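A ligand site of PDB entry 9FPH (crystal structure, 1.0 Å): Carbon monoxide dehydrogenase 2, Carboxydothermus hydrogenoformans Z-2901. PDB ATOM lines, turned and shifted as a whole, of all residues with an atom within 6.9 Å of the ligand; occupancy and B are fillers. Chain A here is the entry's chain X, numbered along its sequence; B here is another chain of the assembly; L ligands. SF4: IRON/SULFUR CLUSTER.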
ATOM      1  N   CYS A  47     -32.127  -4.925  -5.193  1.00  0.00           N
ATOM      2  CA  CYS A  47     -31.030  -4.384  -5.987  1.00  0.00           C
ATOM      3  C   CYS A  47     -30.026  -3.775  -5.030  1.00  0.00           C
ATOM      4  O   CYS A  47     -30.397  -3.140  -4.019  1.00  0.00           O
ATOM      5  CB  CYS A  47     -31.544  -3.337  -6.942  1.00  0.00           C
ATOM      6  SG  CYS A  47     -30.169  -2.592  -7.925  1.00  0.00           S
ATOM      7  N   CYS A  48     -28.746  -3.949  -5.340  1.00  0.00           N
ATOM      8  CA  CYS A  48     -27.646  -3.384  -4.563  1.00  0.00           C
ATOM      9  C   CYS A  48     -26.599  -2.819  -5.513  1.00  0.00           C
ATOM     10  O   CYS A  48     -26.151  -3.492  -6.448  1.00  0.00           O
ATOM     11  CB  CYS A  48     -27.037  -4.435  -3.674  1.00  0.00           C
ATOM     12  SG  CYS A  48     -25.660  -3.789  -2.645  1.00  0.00           S
ATOM     13  N   ARG A  49     -26.166  -1.592  -5.220  1.00  0.00           N
ATOM     14  CA  ARG A  49     -25.110  -0.881  -5.911  1.00  0.00           C
ATOM     15  C   ARG A  49     -24.042  -0.393  -4.921  1.00  0.00           C
ATOM     16  O   ARG A  49     -23.412   0.646  -5.143  1.00  0.00           O
ATOM     17  CB  ARG A  49     -25.653   0.255  -6.769  1.00  0.00           C
ATOM     18  CG  ARG A  49     -26.582  -0.218  -7.844  1.00  0.00           C
ATOM     19  CD  ARG A  49     -27.340   0.921  -8.442  1.00  0.00           C
ATOM     20  NE  ARG A  49     -26.464   1.898  -9.039  1.00  0.00           N
ATOM     21  CZ  ARG A  49     -26.692   3.170  -9.242  1.00  0.00           C
ATOM     22  NH1 ARG A  49     -27.873   3.708  -9.025  1.00  0.00           N
ATOM     23  NH2 ARG A  49     -25.721   3.914  -9.802  1.00  0.00           N
ATOM     24  N   HIS A  50     -23.856  -1.134  -3.830  1.00  0.00           N
ATOM     25  CA  HIS A  50     -22.927  -0.699  -2.794  1.00  0.00           C
ATOM     26  C   HIS A  50     -21.474  -0.972  -3.122  1.00  0.00           C
ATOM     27  O   HIS A  50     -20.616  -0.543  -2.328  1.00  0.00           O
ATOM     28  CB  HIS A  50     -23.314  -1.242  -1.427  1.00  0.00           C
ATOM     29  CG  HIS A  50     -24.621  -0.695  -0.906  1.00  0.00           C
ATOM     30  ND1 HIS A  50     -24.982  -0.792   0.413  1.00  0.00           N
ATOM     31  CD2 HIS A  50     -25.669  -0.074  -1.495  1.00  0.00           C
ATOM     32  CE1 HIS A  50     -26.187  -0.258   0.593  1.00  0.00           C
ATOM     33  NE2 HIS A  50     -26.638   0.200  -0.555  1.00  0.00           N
ATOM     34  N   CYS A  51     -21.135  -1.602  -4.235  1.00  0.00           N
ATOM     35  CA  CYS A  51     -19.740  -1.670  -4.675  1.00  0.00           C
ATOM     36  C   CYS A  51     -19.708  -1.726  -6.192  1.00  0.00           C
ATOM     37  O   CYS A  51     -20.720  -1.912  -6.865  1.00  0.00           O
ATOM     38  CB  CYS A  51     -18.934  -2.765  -4.000  1.00  0.00           C
ATOM     39  SG  CYS A  51     -19.191  -4.414  -4.718  1.00  0.00           S
ATOM     40  N   LEU A  52     -18.460  -1.658  -6.725  1.00  0.00           N
ATOM     41  CA  LEU A  52     -18.235  -1.631  -8.154  1.00  0.00           C
ATOM     42  C   LEU A  52     -18.241  -3.021  -8.792  1.00  0.00           C
ATOM     43  O   LEU A  52     -18.010  -3.131 -10.001  1.00  0.00           O
ATOM     44  CB  LEU A  52     -16.979  -0.848  -8.527  1.00  0.00           C
ATOM     45  CG  LEU A  52     -16.901   0.572  -7.990  1.00  0.00           C
ATOM     46  CD1 LEU A  52     -15.610   1.207  -8.426  1.00  0.00           C
ATOM     47  CD2 LEU A  52     -18.101   1.374  -8.469  1.00  0.00           C
ATOM     48  N   GLN A  53     -18.497  -4.070  -8.016  1.00  0.00           N
ATOM     49  CA  GLN A  53     -18.849  -5.363  -8.596  1.00  0.00           C
ATOM     50  C   GLN A  53     -20.282  -5.384  -9.066  1.00  0.00           C
ATOM     51  O   GLN A  53     -20.636  -6.223  -9.899  1.00  0.00           O
ATOM     52  CB  GLN A  53     -18.570  -6.529  -7.662  1.00  0.00           C
ATOM     53  CG  GLN A  53     -17.094  -6.649  -7.389  1.00  0.00           C
ATOM     54  CD  GLN A  53     -16.642  -7.823  -6.555  1.00  0.00           C
ATOM     55  OE1 GLN A  53     -15.546  -8.336  -6.737  1.00  0.00           O
ATOM     56  NE2 GLN A  53     -17.475  -8.298  -5.670  1.00  0.00           N
ATOM     57  N   GLY A  54     -21.127  -4.507  -8.543  1.00  0.00           N
ATOM     58  CA  GLY A  54     -22.489  -4.420  -8.961  1.00  0.00           C
ATOM     59  C   GLY A  54     -22.655  -3.735 -10.278  1.00  0.00           C
ATOM     60  O   GLY A  54     -21.699  -3.420 -10.969  1.00  0.00           O
ATOM     61  N   PRO A  55     -23.915  -3.508 -10.677  1.00  0.00           N
ATOM     62  CA  PRO A  55     -25.136  -3.708  -9.874  1.00  0.00           C
ATOM     63  C   PRO A  55     -25.491  -5.160  -9.699  1.00  0.00           C
ATOM     64  O   PRO A  55     -25.380  -5.966 -10.625  1.00  0.00           O
ATOM     65  CB  PRO A  55     -26.183  -2.947 -10.687  1.00  0.00           C
ATOM     66  CG  PRO A  55     -25.686  -3.067 -12.124  1.00  0.00           C
ATOM     67  CD  PRO A  55     -24.223  -2.933 -12.001  1.00  0.00           C
ATOM     68  N   CYS A  56     -25.948  -5.513  -8.505  1.00  0.00           N
ATOM     69  CA  CYS A  56     -26.452  -6.817  -8.177  1.00  0.00           C
ATOM     70  C   CYS A  56     -27.965  -6.730  -8.035  1.00  0.00           C
ATOM     71  O   CYS A  56     -28.521  -5.732  -7.580  1.00  0.00           O
ATOM     72  CB  CYS A  56     -25.861  -7.338  -6.889  1.00  0.00           C
ATOM     73  SG  CYS A  56     -24.081  -7.797  -7.087  1.00  0.00           S
ATOM     74  N   ARG A  57     -28.640  -7.823  -8.339  1.00  0.00           N
ATOM     75  CA  ARG A  57     -30.075  -7.969  -8.164  1.00  0.00           C
ATOM     76  C   ARG A  57     -30.383  -9.405  -7.780  1.00  0.00           C
ATOM     77  O   ARG A  57     -29.539 -10.307  -7.960  1.00  0.00           O
ATOM     78  CB  ARG A  57     -30.845  -7.598  -9.442  1.00  0.00           C
ATOM     79  CG  ARG A  57     -30.871  -8.687 -10.496  1.00  0.00           C
ATOM     80  CD  ARG A  57     -30.966  -8.065 -11.870  1.00  0.00           C
ATOM     81  NE  ARG A  57     -30.871  -9.048 -12.932  1.00  0.00           N
ATOM     82  CZ  ARG A  57     -29.782  -9.742 -13.199  1.00  0.00           C
ATOM     83  NH1 ARG A  57     -28.638  -9.432 -12.600  1.00  0.00           N
ATOM     84  NH2 ARG A  57     -29.820 -10.758 -14.029  1.00  0.00           N
ATOM     85  N   VAL A  67     -28.579 -14.435  -5.055  1.00  0.00           N
ATOM     86  CA  VAL A  67     -27.718 -13.871  -4.018  1.00  0.00           C
ATOM     87  C   VAL A  67     -26.809 -12.853  -4.694  1.00  0.00           C
ATOM     88  O   VAL A  67     -26.489 -12.986  -5.877  1.00  0.00           O
ATOM     89  CB  VAL A  67     -26.999 -15.048  -3.328  1.00  0.00           C
ATOM     90  CG1 VAL A  67     -26.089 -15.792  -4.303  1.00  0.00           C
ATOM     91  CG2 VAL A  67     -26.190 -14.603  -2.169  1.00  0.00           C
ATOM     92  N   GLY A  68     -26.393 -11.829  -3.952  1.00  0.00           N
ATOM     93  CA  GLY A  68     -25.454 -10.877  -4.487  1.00  0.00           C
ATOM     94  C   GLY A  68     -24.090 -11.486  -4.730  1.00  0.00           C
ATOM     95  O   GLY A  68     -23.737 -12.549  -4.210  1.00  0.00           O
ATOM     96  N   ILE A  69     -23.251 -10.772  -5.501  1.00  0.00           N
ATOM     97  CA  ILE A  69     -21.953 -11.319  -5.904  1.00  0.00           C
ATOM     98  C   ILE A  69     -21.076 -11.599  -4.681  1.00  0.00           C
ATOM     99  O   ILE A  69     -20.394 -12.635  -4.629  1.00  0.00           O
ATOM    100  CB  ILE A  69     -21.275 -10.392  -6.936  1.00  0.00           C
ATOM    101  CG1 ILE A  69     -22.044 -10.486  -8.267  1.00  0.00           C
ATOM    102  CG2 ILE A  69     -19.812 -10.747  -7.104  1.00  0.00           C
ATOM    103  CD1 ILE A  69     -21.611  -9.473  -9.302  1.00  0.00           C
ATOM    104  N   CYS A  70     -21.065 -10.706  -3.676  1.00  0.00           N
ATOM    105  CA  CYS A  70     -20.292 -10.916  -2.461  1.00  0.00           C
ATOM    106  C   CYS A  70     -20.891 -11.948  -1.514  1.00  0.00           C
ATOM    107  O   CYS A  70     -20.297 -12.256  -0.485  1.00  0.00           O
ATOM    108  CB  CYS A  70     -20.109  -9.593  -1.723  1.00  0.00           C
ATOM    109  SG  CYS A  70     -21.749  -8.936  -1.194  1.00  0.00           S
ATOM    110  N   GLY A  71     -22.080 -12.472  -1.823  1.00  0.00           N
ATOM    111  CA  GLY A  71     -22.816 -13.340  -0.940  1.00  0.00           C
ATOM    112  C   GLY A  71     -23.949 -12.687  -0.199  1.00  0.00           C
ATOM    113  O   GLY A  71     -24.617 -13.353   0.629  1.00  0.00           O
ATOM    114  N   ALA A  72     -24.187 -11.385  -0.403  1.00  0.00           N
ATOM    115  CA  ALA A  72     -25.263 -10.695   0.315  1.00  0.00           C
ATOM    116  C   ALA A  72     -26.620 -11.298  -0.045  1.00  0.00           C
ATOM    117  O   ALA A  72     -26.985 -11.392  -1.219  1.00  0.00           O
ATOM    118  CB  ALA A  72     -25.245  -9.222  -0.035  1.00  0.00           C
ATOM    119  N   THR A  73     -27.370 -11.707   0.963  1.00  0.00           N
ATOM    120  CA  THR A  73     -28.692 -12.303   0.773  1.00  0.00           C
ATOM    121  C   THR A  73     -29.734 -11.219   0.527  1.00  0.00           C
ATOM    122  O   THR A  73     -29.508 -10.006   0.709  1.00  0.00           O
ATOM    123  CB  THR A  73     -29.117 -13.102   1.988  1.00  0.00           C
ATOM    124  OG1 THR A  73     -29.172 -12.161   3.070  1.00  0.00           O
ATOM    125  CG2 THR A  73     -28.151 -14.254   2.273  1.00  0.00           C
ATOM    126  N   ILE A  77     -29.526  -7.276   1.652  1.00  0.00           N
ATOM    127  CA  ILE A  77     -29.656  -6.198   0.669  1.00  0.00           C
ATOM    128  C   ILE A  77     -30.835  -5.283   1.029  1.00  0.00           C
ATOM    129  O   ILE A  77     -30.712  -4.055   1.047  1.00  0.00           O
ATOM    130  CB  ILE A  77     -29.746  -6.778  -0.760  1.00  0.00           C
ATOM    131  CG1 ILE A  77     -28.355  -7.308  -1.165  1.00  0.00           C
ATOM    132  CG2 ILE A  77     -30.355  -5.810  -1.710  1.00  0.00           C
ATOM    133  CD1 ILE A  77     -28.423  -8.096  -2.500  1.00  0.00           C
ATOM    134  N   ARG A  80     -30.036  -3.251   4.237  1.00  0.00           N
ATOM    135  CA  ARG A  80     -29.029  -2.214   4.035  1.00  0.00           C
ATOM    136  C   ARG A  80     -29.602  -1.019   3.293  1.00  0.00           C
ATOM    137  O   ARG A  80     -29.322   0.129   3.616  1.00  0.00           O
ATOM    138  CB  ARG A  80     -27.806  -2.761   3.276  1.00  0.00           C
ATOM    139  CG  ARG A  80     -27.017  -3.809   4.043  1.00  0.00           C
ATOM    140  CD  ARG A  80     -25.650  -4.151   3.456  1.00  0.00           C
ATOM    141  NE  ARG A  80     -25.764  -4.600   2.060  1.00  0.00           N
ATOM    142  CZ  ARG A  80     -24.767  -5.199   1.422  1.00  0.00           C
ATOM    143  NH1 ARG A  80     -23.640  -5.471   2.049  1.00  0.00           N
ATOM    144  NH2 ARG A  80     -24.914  -5.563   0.152  1.00  0.00           N
ATOM    145  N   THR A 197     -23.477  -0.549   6.407  1.00  0.00           N
ATOM    146  CA  THR A 197     -24.164  -0.927   5.201  1.00  0.00           C
ATOM    147  C   THR A 197     -23.258  -0.966   3.970  1.00  0.00           C
ATOM    148  O   THR A 197     -23.710  -1.416   2.891  1.00  0.00           O
ATOM    149  CB  THR A 197     -25.375  -0.017   4.912  1.00  0.00           C
ATOM    150  OG1 THR A 197     -24.910   1.307   4.741  1.00  0.00           O
ATOM    151  CG2 THR A 197     -26.438  -0.133   5.996  1.00  0.00           C
ATOM    152  N   SER A 198     -22.001  -0.550   4.100  1.00  0.00           N
ATOM    153  CA  SER A 198     -21.061  -0.657   2.997  1.00  0.00           C
ATOM    154  C   SER A 198     -20.634  -2.116   2.821  1.00  0.00           C
ATOM    155  O   SER A 198     -20.937  -3.006   3.646  1.00  0.00           O
ATOM    156  CB  SER A 198     -19.874   0.255   3.243  1.00  0.00           C
ATOM    157  OG  SER A 198     -18.960  -0.190   4.211  1.00  0.00           O
ATOM    158  N   MET A 199     -19.961  -2.404   1.711  1.00  0.00           N
ATOM    159  CA  MET A 199     -19.699  -3.790   1.364  1.00  0.00           C
ATOM    160  C   MET A 199     -18.845  -4.490   2.428  1.00  0.00           C
ATOM    161  O   MET A 199     -17.870  -3.927   2.961  1.00  0.00           O
ATOM    162  CB  MET A 199     -19.050  -3.886  -0.018  1.00  0.00           C
ATOM    163  CG  MET A 199     -18.752  -5.289  -0.509  1.00  0.00           C
ATOM    164  SD  MET A 199     -17.158  -5.841   0.128  1.00  0.00           S
ATOM    165  CE  MET A 199     -17.176  -7.573  -0.294  1.00  0.00           C
ATOM    166  N   GLY A 200     -19.245  -5.719   2.726  1.00  0.00           N
ATOM    167  CA  GLY A 200     -18.423  -6.541   3.565  1.00  0.00           C
ATOM    168  C   GLY A 200     -18.432  -6.189   5.027  1.00  0.00           C
ATOM    169  O   GLY A 200     -17.485  -6.527   5.763  1.00  0.00           O
ATOM    170  N   VAL B  28     -17.408 -16.534  -5.355  1.00  0.00           N
ATOM    171  CA  VAL B  28     -17.684 -15.191  -5.895  1.00  0.00           C
ATOM    172  C   VAL B  28     -17.750 -15.205  -7.405  1.00  0.00           C
ATOM    173  O   VAL B  28     -18.564 -14.494  -7.991  1.00  0.00           O
ATOM    174  CB  VAL B  28     -16.668 -14.181  -5.329  1.00  0.00           C
ATOM    175  CG1 VAL B  28     -15.236 -14.522  -5.781  1.00  0.00           C
ATOM    176  CG2 VAL B  28     -17.030 -12.766  -5.660  1.00  0.00           C
ATOM    177  N   MET B  35     -25.051 -13.539 -12.161  1.00  0.00           N
ATOM    178  CA  MET B  35     -25.583 -12.172 -12.208  1.00  0.00           C
ATOM    179  C   MET B  35     -25.640 -11.604 -13.628  1.00  0.00           C
ATOM    180  O   MET B  35     -26.228 -10.562 -13.853  1.00  0.00           O
ATOM    181  CB  MET B  35     -24.711 -11.318 -11.228  1.00  0.00           C
ATOM    182  CG  MET B  35     -25.436  -9.975 -10.922  1.00  0.00           C
ATOM    183  SD  MET B  35     -26.897 -10.268  -9.851  1.00  0.00           S
ATOM    184  CE  MET B  35     -26.213 -11.064  -8.398  1.00  0.00           C
ATOM    185  N   GLN B  38     -25.536  -7.941 -16.213  1.00  0.00           N
ATOM    186  CA  GLN B  38     -25.872  -6.981 -15.167  1.00  0.00           C
ATOM    187  C   GLN B  38     -26.682  -5.808 -15.750  1.00  0.00           C
ATOM    188  O   GLN B  38     -26.655  -5.510 -16.941  1.00  0.00           O
ATOM    189  CB  GLN B  38     -24.605  -6.489 -14.458  1.00  0.00           C
ATOM    190  CG  GLN B  38     -23.946  -7.595 -13.672  1.00  0.00           C
ATOM    191  CD  GLN B  38     -22.696  -7.190 -12.978  1.00  0.00           C
ATOM    192  OE1 GLN B  38     -21.640  -7.167 -13.597  1.00  0.00           O
ATOM    193  NE2 GLN B  38     -22.786  -6.875 -11.695  1.00  0.00           N
ATOM    194  N   PRO B 336     -19.848 -11.900   2.769  1.00  0.00           N
ATOM    195  CA  PRO B 336     -20.655 -12.616   3.754  1.00  0.00           C
ATOM    196  C   PRO B 336     -20.862 -14.078   3.415  1.00  0.00           C
ATOM    197  O   PRO B 336     -21.234 -14.889   4.273  1.00  0.00           O
ATOM    198  CB  PRO B 336     -21.954 -11.805   3.844  1.00  0.00           C
ATOM    199  CG  PRO B 336     -22.021 -11.087   2.524  1.00  0.00           C
ATOM    200  CD  PRO B 336     -20.578 -10.747   2.201  1.00  0.00           C
ATOM    201  N   MET B 560     -13.077  -1.807  -6.167  1.00  0.00           N
ATOM    202  CA  MET B 560     -14.355  -2.437  -5.803  1.00  0.00           C
ATOM    203  C   MET B 560     -15.078  -1.582  -4.792  1.00  0.00           C
ATOM    204  O   MET B 560     -16.260  -1.235  -5.012  1.00  0.00           O
ATOM    205  CB  MET B 560     -14.123  -3.881  -5.307  1.00  0.00           C
ATOM    206  CG  MET B 560     -15.334  -4.663  -4.904  1.00  0.00           C
ATOM    207  SD  MET B 560     -15.753  -4.482  -3.113  1.00  0.00           S
ATOM    208  CE  MET B 560     -14.298  -5.134  -2.325  1.00  0.00           C
HETATM  209 FE1  SF4 L   1     -23.152  -6.775  -5.241  1.00  0.00          FE
HETATM  210 FE2  SF4 L   1     -21.285  -5.151  -4.169  1.00  0.00          FE
HETATM  211 FE3  SF4 L   1     -23.845  -5.056  -3.304  1.00  0.00          FE
HETATM  212 FE4  SF4 L   1     -22.338  -7.234  -2.670  1.00  0.00          FE
HETATM  213  S1  SF4 L   1     -22.036  -5.039  -1.957  1.00  0.00           S
HETATM  214  S2  SF4 L   1     -24.477  -7.280  -3.384  1.00  0.00           S
HETATM  215  S3  SF4 L   1     -21.077  -7.432  -4.632  1.00  0.00           S
HETATM  216  S4  SF4 L   1     -23.064  -4.450  -5.381  1.00  0.00           S
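A sulfur (S4) of the ligand lies close to the backbone NH (N) of Cys 51 (3.6 Å).
FE2 of the ligand is bound by SG of Cys 51 (2.3 Å).
An iron atom (FE1) of the ligand is bound by the side-chain sulfur (SG) of Cys 56 (2.3 Å).
SG of Cys 48 is bound to FE3 of the ligand (2.3 Å).
S3 of the ligand sits close to N of Cys 70.
An iron atom (FE4) of the ligand is bound by the side-chain sulfur (SG) of Cys 70 (2.3 Å).
The guanidinium group of Arg 80 lies close to a sulfur (S1) of the ligand, 3.6 Å away.
The backbone NH (N) of Gly 54 sits close to a sulfur (S4) of the ligand (3.7 Å).
S4 of the ligand lies close to N of His 50, 3.7 Å away.
SG of Cys 51 sits close to N of Gln 53, at 3.4 Å.
SD of Met 560 of chain B lies close to SG of Cys 51 (3.8 Å).
O of Cys 56 is in hydrogen-bond range of N of Cys 48 (2.9 Å).
SG of Cys 56 sits close to N of Ile 69 (3.5 Å).
The backbone carbonyl oxygen of Cys 56 sits close to the side-chain sulfur of Cys 47 (3.6 Å).
NH2 of Arg 80 lies close to SG of Cys 48.
The side-chain sulfur (SG) of Cys 70 sits close to the backbone NH (N) of Ala 72, 3.5 Å away.
The side-chain amide nitrogen (NE2) of Gln 38 of chain B sits at hydrogen-bond distance from the backbone carbonyl oxygen (O) of Gln 53 (2.9 Å).
Residues that only touch the ligand: Met 199 (3.6 Å), Ile 69 (3.8 Å), Gln 53 (3.8 Å), Gly 68 (3.9 Å) and Ala 72 (3.9 Å).
The nearest printed residue that does not touch the ligand is Ile 77 (4.1 Å).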
